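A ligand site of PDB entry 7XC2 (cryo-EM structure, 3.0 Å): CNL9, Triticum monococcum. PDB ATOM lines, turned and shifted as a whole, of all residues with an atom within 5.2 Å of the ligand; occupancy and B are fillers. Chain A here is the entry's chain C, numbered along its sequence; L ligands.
Merely in contact with the ligand: Ala 139 (3.7 Å), Glu 146 (3.7 Å), Leu 147 (3.6 Å), Ile 150 (3.9 Å), Gly 181 (3.7 Å), Leu 183 (3.8 Å), Pro 350 (3.7 Å) and Ile 354 (3.8 Å). Hydrophobic or aromatic side chains that line the ligand: Ala 139, Leu 147, Ile 150, Pro 350 and Ile 354. 16 residues have an atom within 4 Å of the ligand: Arg 136, Ala 139, Glu 146, Leu 147, Val 148, Ile 150, Gly 181, Gly 182, Leu 183, Gly 184, Lys 185, Thr 186, Thr 187, Arg 290, Pro 350 and Ile 354.
The backbone NH (N) of Thr 187 sits at hydrogen-bond distance from an oxygen (O8) of the ligand (3.3 Å). The side-chain hydroxyl (OG1) of Thr 187 sits at hydrogen-bond distance from an oxygen (O8) of the ligand, 2.7 Å away. O4 of the ligand is in hydrogen-bond range of N of Lys 185 (2.9 Å). The side-chain amino group (NZ) of Lys 185 is in salt-bridge range of an oxygen (O4) of the ligand (2.8 Å). O3 of the ligand is in salt-bridge range of NH2 of Arg 290 (2.9 Å). N of Gly 184 sits at hydrogen-bond distance from O9 of the ligand, 3.0 Å away. The side-chain hydroxyl (OG1) of Thr 186 lies within hydrogen-bond range of an oxygen (O8) of the ligand, at 3.1 Å. An oxygen (O6) of the ligand lies within hydrogen-bond range of the backbone NH (N) of Gly 182, at 3.2 Å. N of Val 148 sits at hydrogen-bond distance from N4 of the ligand. NH1 of Arg 136 is in salt-bridge range of O2 of the ligand, 3.3 Å away.
NZ of Lys 185 is in hydrogen-bond range of O of Phe 180, 3.1 Å away. O of Gly 182 lies within hydrogen-bond range of N of Leu 351 (3.5 Å).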
ATOM      1  N   ARG A 136      -0.007  -9.879 -14.123  1.00  0.00           N
ATOM      2  CA  ARG A 136       0.876 -11.028 -14.246  1.00  0.00           C
ATOM      3  C   ARG A 136       1.273 -11.310 -15.683  1.00  0.00           C
ATOM      4  O   ARG A 136       2.048 -12.233 -15.922  1.00  0.00           O
ATOM      5  CB  ARG A 136       0.201 -12.271 -13.672  1.00  0.00           C
ATOM      6  CG  ARG A 136      -0.073 -12.191 -12.203  1.00  0.00           C
ATOM      7  CD  ARG A 136      -0.839 -13.398 -11.760  1.00  0.00           C
ATOM      8  NE  ARG A 136      -2.176 -13.425 -12.320  1.00  0.00           N
ATOM      9  CZ  ARG A 136      -3.046 -14.399 -12.111  1.00  0.00           C
ATOM     10  NH1 ARG A 136      -2.719 -15.426 -11.350  1.00  0.00           N
ATOM     11  NH2 ARG A 136      -4.249 -14.344 -12.656  1.00  0.00           N
ATOM     12  N   ALA A 139       5.142 -10.622 -16.800  1.00  0.00           N
ATOM     13  CA  ALA A 139       6.167 -11.533 -16.306  1.00  0.00           C
ATOM     14  C   ALA A 139       6.542 -12.592 -17.331  1.00  0.00           C
ATOM     15  O   ALA A 139       7.611 -13.186 -17.220  1.00  0.00           O
ATOM     16  CB  ALA A 139       5.711 -12.196 -15.018  1.00  0.00           C
ATOM     17  N   THR A 142       9.824 -11.573 -19.218  1.00  0.00           N
ATOM     18  CA  THR A 142      11.062 -11.398 -18.489  1.00  0.00           C
ATOM     19  C   THR A 142      12.169 -12.206 -19.153  1.00  0.00           C
ATOM     20  O   THR A 142      11.955 -13.340 -19.586  1.00  0.00           O
ATOM     21  CB  THR A 142      10.893 -11.829 -17.038  1.00  0.00           C
ATOM     22  OG1 THR A 142      10.081 -10.861 -16.350  1.00  0.00           O
ATOM     23  CG2 THR A 142      12.224 -11.953 -16.333  1.00  0.00           C
ATOM     24  N   GLU A 146      17.807 -13.905 -16.023  1.00  0.00           N
ATOM     25  CA  GLU A 146      17.587 -13.275 -14.727  1.00  0.00           C
ATOM     26  C   GLU A 146      16.941 -14.206 -13.729  1.00  0.00           C
ATOM     27  O   GLU A 146      16.549 -13.758 -12.642  1.00  0.00           O
ATOM     28  CB  GLU A 146      16.732 -12.024 -14.904  1.00  0.00           C
ATOM     29  CG  GLU A 146      17.416 -10.956 -15.704  1.00  0.00           C
ATOM     30  CD  GLU A 146      16.805  -9.599 -15.466  1.00  0.00           C
ATOM     31  OE1 GLU A 146      15.696  -9.534 -14.907  1.00  0.00           O
ATOM     32  OE2 GLU A 146      17.440  -8.586 -15.835  1.00  0.00           O
ATOM     33  N   LEU A 147      16.813 -15.483 -14.042  1.00  0.00           N
ATOM     34  CA  LEU A 147      16.270 -16.455 -13.112  1.00  0.00           C
ATOM     35  C   LEU A 147      17.418 -17.163 -12.415  1.00  0.00           C
ATOM     36  O   LEU A 147      18.400 -17.554 -13.047  1.00  0.00           O
ATOM     37  CB  LEU A 147      15.380 -17.453 -13.834  1.00  0.00           C
ATOM     38  CG  LEU A 147      14.378 -16.824 -14.800  1.00  0.00           C
ATOM     39  CD1 LEU A 147      13.497 -17.892 -15.373  1.00  0.00           C
ATOM     40  CD2 LEU A 147      13.553 -15.780 -14.097  1.00  0.00           C
ATOM     41  N   VAL A 148      17.278 -17.352 -11.105  1.00  0.00           N
ATOM     42  CA  VAL A 148      18.430 -17.740 -10.292  1.00  0.00           C
ATOM     43  C   VAL A 148      18.551 -19.246 -10.161  1.00  0.00           C
ATOM     44  O   VAL A 148      19.541 -19.844 -10.583  1.00  0.00           O
ATOM     45  CB  VAL A 148      18.367 -17.082  -8.911  1.00  0.00           C
ATOM     46  CG1 VAL A 148      19.433 -17.655  -8.027  1.00  0.00           C
ATOM     47  CG2 VAL A 148      18.559 -15.597  -9.038  1.00  0.00           C
ATOM     48  N   GLY A 149      17.555 -19.881  -9.551  1.00  0.00           N
ATOM     49  CA  GLY A 149      17.732 -21.266  -9.162  1.00  0.00           C
ATOM     50  C   GLY A 149      16.807 -22.270  -9.812  1.00  0.00           C
ATOM     51  O   GLY A 149      16.270 -23.139  -9.118  1.00  0.00           O
ATOM     52  N   ILE A 150      16.597 -22.166 -11.118  1.00  0.00           N
ATOM     53  CA  ILE A 150      15.610 -23.026 -11.756  1.00  0.00           C
ATOM     54  C   ILE A 150      16.146 -24.415 -12.102  1.00  0.00           C
ATOM     55  O   ILE A 150      15.402 -25.394 -11.980  1.00  0.00           O
ATOM     56  CB  ILE A 150      15.028 -22.346 -13.002  1.00  0.00           C
ATOM     57  CG1 ILE A 150      16.154 -21.867 -13.902  1.00  0.00           C
ATOM     58  CG2 ILE A 150      14.098 -21.219 -12.622  1.00  0.00           C
ATOM     59  CD1 ILE A 150      15.670 -21.342 -15.223  1.00  0.00           C
ATOM     60  N   PHE A 180       1.178 -21.071  -3.181  1.00  0.00           N
ATOM     61  CA  PHE A 180       0.586 -19.758  -3.026  1.00  0.00           C
ATOM     62  C   PHE A 180       1.051 -18.824  -4.142  1.00  0.00           C
ATOM     63  O   PHE A 180       1.922 -19.163  -4.940  1.00  0.00           O
ATOM     64  CB  PHE A 180       0.913 -19.159  -1.662  1.00  0.00           C
ATOM     65  CG  PHE A 180       0.056 -17.992  -1.309  1.00  0.00           C
ATOM     66  CD1 PHE A 180      -1.273 -17.940  -1.697  1.00  0.00           C
ATOM     67  CD2 PHE A 180       0.574 -16.924  -0.590  1.00  0.00           C
ATOM     68  CE1 PHE A 180      -2.065 -16.864  -1.384  1.00  0.00           C
ATOM     69  CE2 PHE A 180      -0.218 -15.839  -0.281  1.00  0.00           C
ATOM     70  CZ  PHE A 180      -1.537 -15.814  -0.675  1.00  0.00           C
ATOM     71  N   GLY A 181       0.460 -17.635  -4.180  1.00  0.00           N
ATOM     72  CA  GLY A 181       0.761 -16.702  -5.244  1.00  0.00           C
ATOM     73  C   GLY A 181       2.170 -16.153  -5.147  1.00  0.00           C
ATOM     74  O   GLY A 181       2.741 -16.007  -4.072  1.00  0.00           O
ATOM     75  N   GLY A 182       2.728 -15.821  -6.306  1.00  0.00           N
ATOM     76  CA  GLY A 182       4.065 -15.278  -6.356  1.00  0.00           C
ATOM     77  C   GLY A 182       5.165 -16.263  -6.128  1.00  0.00           C
ATOM     78  O   GLY A 182       6.311 -15.862  -5.923  1.00  0.00           O
ATOM     79  N   LEU A 183       4.872 -17.555  -6.159  1.00  0.00           N
ATOM     80  CA  LEU A 183       5.863 -18.569  -5.841  1.00  0.00           C
ATOM     81  C   LEU A 183       6.704 -18.988  -7.034  1.00  0.00           C
ATOM     82  O   LEU A 183       7.814 -19.494  -6.839  1.00  0.00           O
ATOM     83  CB  LEU A 183       5.173 -19.790  -5.250  1.00  0.00           C
ATOM     84  CG  LEU A 183       5.979 -20.605  -4.243  1.00  0.00           C
ATOM     85  CD1 LEU A 183       6.725 -19.688  -3.320  1.00  0.00           C
ATOM     86  CD2 LEU A 183       5.037 -21.468  -3.460  1.00  0.00           C
ATOM     87  N   GLY A 184       6.203 -18.816  -8.252  1.00  0.00           N
ATOM     88  CA  GLY A 184       6.990 -19.153  -9.420  1.00  0.00           C
ATOM     89  C   GLY A 184       6.516 -20.386 -10.150  1.00  0.00           C
ATOM     90  O   GLY A 184       7.327 -21.149 -10.662  1.00  0.00           O
ATOM     91  N   LYS A 185       5.197 -20.596 -10.218  1.00  0.00           N
ATOM     92  CA  LYS A 185       4.678 -21.790 -10.855  1.00  0.00           C
ATOM     93  C   LYS A 185       4.687 -21.678 -12.365  1.00  0.00           C
ATOM     94  O   LYS A 185       5.258 -22.528 -13.064  1.00  0.00           O
ATOM     95  CB  LYS A 185       3.273 -22.079 -10.345  1.00  0.00           C
ATOM     96  CG  LYS A 185       3.193 -22.243  -8.852  1.00  0.00           C
ATOM     97  CD  LYS A 185       1.814 -22.645  -8.408  1.00  0.00           C
ATOM     98  CE  LYS A 185       0.841 -21.516  -8.567  1.00  0.00           C
ATOM     99  NZ  LYS A 185       1.155 -20.405  -7.651  1.00  0.00           N
ATOM    100  N   THR A 186       4.069 -20.628 -12.908  1.00  0.00           N
ATOM    101  CA  THR A 186       4.003 -20.488 -14.351  1.00  0.00           C
ATOM    102  C   THR A 186       5.390 -20.278 -14.947  1.00  0.00           C
ATOM    103  O   THR A 186       5.632 -20.677 -16.079  1.00  0.00           O
ATOM    104  CB  THR A 186       3.098 -19.336 -14.742  1.00  0.00           C
ATOM    105  OG1 THR A 186       3.767 -18.106 -14.499  1.00  0.00           O
ATOM    106  CG2 THR A 186       1.842 -19.358 -13.928  1.00  0.00           C
ATOM    107  N   THR A 187       6.310 -19.692 -14.190  1.00  0.00           N
ATOM    108  CA  THR A 187       7.681 -19.559 -14.675  1.00  0.00           C
ATOM    109  C   THR A 187       8.308 -20.920 -14.899  1.00  0.00           C
ATOM    110  O   THR A 187       8.936 -21.160 -15.936  1.00  0.00           O
ATOM    111  CB  THR A 187       8.506 -18.762 -13.675  1.00  0.00           C
ATOM    112  OG1 THR A 187       7.922 -17.474 -13.501  1.00  0.00           O
ATOM    113  CG2 THR A 187       9.906 -18.598 -14.185  1.00  0.00           C
ATOM    114  N   ARG A 290      -3.649 -22.525  -7.506  1.00  0.00           N
ATOM    115  CA  ARG A 290      -3.469 -22.171  -6.103  1.00  0.00           C
ATOM    116  C   ARG A 290      -4.291 -23.030  -5.153  1.00  0.00           C
ATOM    117  O   ARG A 290      -4.070 -22.970  -3.942  1.00  0.00           O
ATOM    118  CB  ARG A 290      -3.847 -20.713  -5.849  1.00  0.00           C
ATOM    119  CG  ARG A 290      -2.787 -19.695  -6.155  1.00  0.00           C
ATOM    120  CD  ARG A 290      -3.233 -18.325  -5.687  1.00  0.00           C
ATOM    121  NE  ARG A 290      -2.537 -17.247  -6.380  1.00  0.00           N
ATOM    122  CZ  ARG A 290      -2.767 -15.960  -6.160  1.00  0.00           C
ATOM    123  NH1 ARG A 290      -3.666 -15.597  -5.275  1.00  0.00           N
ATOM    124  NH2 ARG A 290      -2.092 -15.048  -6.827  1.00  0.00           N
ATOM    125  N   LEU A 311      12.466 -20.666  -2.065  1.00  0.00           N
ATOM    126  CA  LEU A 311      13.901 -20.804  -2.243  1.00  0.00           C
ATOM    127  C   LEU A 311      14.592 -20.939  -0.897  1.00  0.00           C
ATOM    128  O   LEU A 311      14.068 -20.583   0.155  1.00  0.00           O
ATOM    129  CB  LEU A 311      14.452 -19.597  -2.982  1.00  0.00           C
ATOM    130  CG  LEU A 311      13.807 -19.242  -4.314  1.00  0.00           C
ATOM    131  CD1 LEU A 311      14.311 -17.911  -4.797  1.00  0.00           C
ATOM    132  CD2 LEU A 311      14.117 -20.312  -5.322  1.00  0.00           C
ATOM    133  N   LEU A 319      19.844 -13.835  -5.295  1.00  0.00           N
ATOM    134  CA  LEU A 319      18.858 -13.117  -6.090  1.00  0.00           C
ATOM    135  C   LEU A 319      18.765 -11.664  -5.650  1.00  0.00           C
ATOM    136  O   LEU A 319      18.773 -10.742  -6.478  1.00  0.00           O
ATOM    137  CB  LEU A 319      17.494 -13.793  -5.971  1.00  0.00           C
ATOM    138  CG  LEU A 319      16.305 -13.078  -6.594  1.00  0.00           C
ATOM    139  CD1 LEU A 319      16.567 -12.761  -8.040  1.00  0.00           C
ATOM    140  CD2 LEU A 319      15.090 -13.934  -6.463  1.00  0.00           C
ATOM    141  N   ARG A 323      19.890  -8.517  -8.012  1.00  0.00           N
ATOM    142  CA  ARG A 323      18.887  -7.512  -8.346  1.00  0.00           C
ATOM    143  C   ARG A 323      19.305  -6.081  -7.997  1.00  0.00           C
ATOM    144  O   ARG A 323      19.044  -5.146  -8.756  1.00  0.00           O
ATOM    145  CB  ARG A 323      17.545  -7.851  -7.691  1.00  0.00           C
ATOM    146  CG  ARG A 323      16.367  -7.089  -8.266  1.00  0.00           C
ATOM    147  CD  ARG A 323      16.348  -7.193  -9.781  1.00  0.00           C
ATOM    148  NE  ARG A 323      16.367  -8.575 -10.242  1.00  0.00           N
ATOM    149  CZ  ARG A 323      15.287  -9.264 -10.601  1.00  0.00           C
ATOM    150  NH1 ARG A 323      14.091  -8.692 -10.547  1.00  0.00           N
ATOM    151  NH2 ARG A 323      15.398 -10.519 -11.007  1.00  0.00           N
ATOM    152  N   PRO A 350       9.783 -15.382  -4.338  1.00  0.00           N
ATOM    153  CA  PRO A 350      10.461 -14.495  -5.290  1.00  0.00           C
ATOM    154  C   PRO A 350       9.763 -13.182  -5.531  1.00  0.00           C
ATOM    155  O   PRO A 350      10.438 -12.173  -5.753  1.00  0.00           O
ATOM    156  CB  PRO A 350      10.512 -15.343  -6.562  1.00  0.00           C
ATOM    157  CG  PRO A 350      10.500 -16.716  -6.078  1.00  0.00           C
ATOM    158  CD  PRO A 350       9.619 -16.733  -4.882  1.00  0.00           C
ATOM    159  N   LEU A 351       8.431 -13.150  -5.504  1.00  0.00           N
ATOM    160  CA  LEU A 351       7.725 -11.904  -5.765  1.00  0.00           C
ATOM    161  C   LEU A 351       8.085 -10.840  -4.740  1.00  0.00           C
ATOM    162  O   LEU A 351       8.414  -9.701  -5.087  1.00  0.00           O
ATOM    163  CB  LEU A 351       6.228 -12.149  -5.785  1.00  0.00           C
ATOM    164  CG  LEU A 351       5.358 -10.972  -6.232  1.00  0.00           C
ATOM    165  CD1 LEU A 351       5.734 -10.565  -7.628  1.00  0.00           C
ATOM    166  CD2 LEU A 351       3.899 -11.349  -6.155  1.00  0.00           C
ATOM    167  N   ILE A 354      11.749  -9.632  -5.095  1.00  0.00           N
ATOM    168  CA  ILE A 354      11.946  -8.742  -6.229  1.00  0.00           C
ATOM    169  C   ILE A 354      11.377  -7.365  -5.949  1.00  0.00           C
ATOM    170  O   ILE A 354      12.011  -6.341  -6.233  1.00  0.00           O
ATOM    171  CB  ILE A 354      11.344  -9.369  -7.493  1.00  0.00           C
ATOM    172  CG1 ILE A 354      12.255 -10.473  -8.003  1.00  0.00           C
ATOM    173  CG2 ILE A 354      11.106  -8.329  -8.544  1.00  0.00           C
ATOM    174  CD1 ILE A 354      11.687 -11.201  -9.176  1.00  0.00           C
ATOM    175  N   ILE A 395      -1.924  -8.282  -6.878  1.00  0.00           N
ATOM    176  CA  ILE A 395      -1.800  -9.695  -7.216  1.00  0.00           C
ATOM    177  C   ILE A 395      -2.197 -10.565  -6.038  1.00  0.00           C
ATOM    178  O   ILE A 395      -2.929 -11.540  -6.186  1.00  0.00           O
ATOM    179  CB  ILE A 395      -0.371 -10.006  -7.682  1.00  0.00           C
ATOM    180  CG1 ILE A 395      -0.163  -9.515  -9.102  1.00  0.00           C
ATOM    181  CG2 ILE A 395      -0.116 -11.476  -7.603  1.00  0.00           C
ATOM    182  CD1 ILE A 395       1.220  -9.750  -9.600  1.00  0.00           C
HETATM  183  P1  LIG L   1       0.408 -16.817  -9.460  1.00  0.00           P
HETATM  184  O1  LIG L   1       0.045 -18.013  -8.644  1.00  0.00           O
HETATM  185  O2  LIG L   1       0.184 -16.979 -10.930  1.00  0.00           O
HETATM  186  O3  LIG L   1      -0.085 -15.517  -8.891  1.00  0.00           O
HETATM  187  P2  LIG L   1       2.955 -17.755 -10.027  1.00  0.00           P
HETATM  188  O4  LIG L   1       2.961 -19.029  -9.245  1.00  0.00           O
HETATM  189  O5  LIG L   1       2.628 -17.758 -11.481  1.00  0.00           O
HETATM  190  O6  LIG L   1       1.994 -16.717  -9.303  1.00  0.00           O
HETATM  191  P3  LIG L   1       5.021 -16.303 -11.114  1.00  0.00           P
HETATM  192  O7  LIG L   1       4.011 -15.285 -11.551  1.00  0.00           O
HETATM  193  O8  LIG L   1       5.579 -17.248 -12.122  1.00  0.00           O
HETATM  194  O9  LIG L   1       4.388 -17.087  -9.874  1.00  0.00           O
HETATM  195  O10 LIG L   1       6.226 -15.504 -10.446  1.00  0.00           O
HETATM  196  C1  LIG L   1       6.068 -14.128 -10.137  1.00  0.00           C
HETATM  197  C2  LIG L   1       7.404 -13.429 -10.300  1.00  0.00           C
HETATM  198  O11 LIG L   1       8.431 -14.174  -9.661  1.00  0.00           O
HETATM  199  C3  LIG L   1       7.778 -13.361 -11.760  1.00  0.00           C
HETATM  200  O12 LIG L   1       7.921 -11.995 -12.116  1.00  0.00           O
HETATM  201  C4  LIG L   1       9.129 -14.017 -11.878  1.00  0.00           C
HETATM  202  O13 LIG L   1       9.981 -13.134 -12.586  1.00  0.00           O
HETATM  203  C5  LIG L   1       9.596 -14.149 -10.455  1.00  0.00           C
HETATM  204  N1  LIG L   1      10.353 -15.402 -10.289  1.00  0.00           N
HETATM  205  C6  LIG L   1       9.824 -16.615 -10.122  1.00  0.00           C
HETATM  206  N2  LIG L   1      10.795 -17.541  -9.984  1.00  0.00           N
HETATM  207  C7  LIG L   1      11.969 -16.918 -10.065  1.00  0.00           C
HETATM  208  C8  LIG L   1      13.374 -17.304 -10.008  1.00  0.00           C
HETATM  209  N3  LIG L   1      13.740 -18.589  -9.826  1.00  0.00           N
HETATM  210  N4  LIG L   1      14.298 -16.344 -10.134  1.00  0.00           N
HETATM  211  C9  LIG L   1      13.955 -15.058 -10.314  1.00  0.00           C
HETATM  212  N5  LIG L   1      12.685 -14.638 -10.382  1.00  0.00           N
HETATM  213  C10 LIG L   1      11.663 -15.507 -10.263  1.00  0.00           C
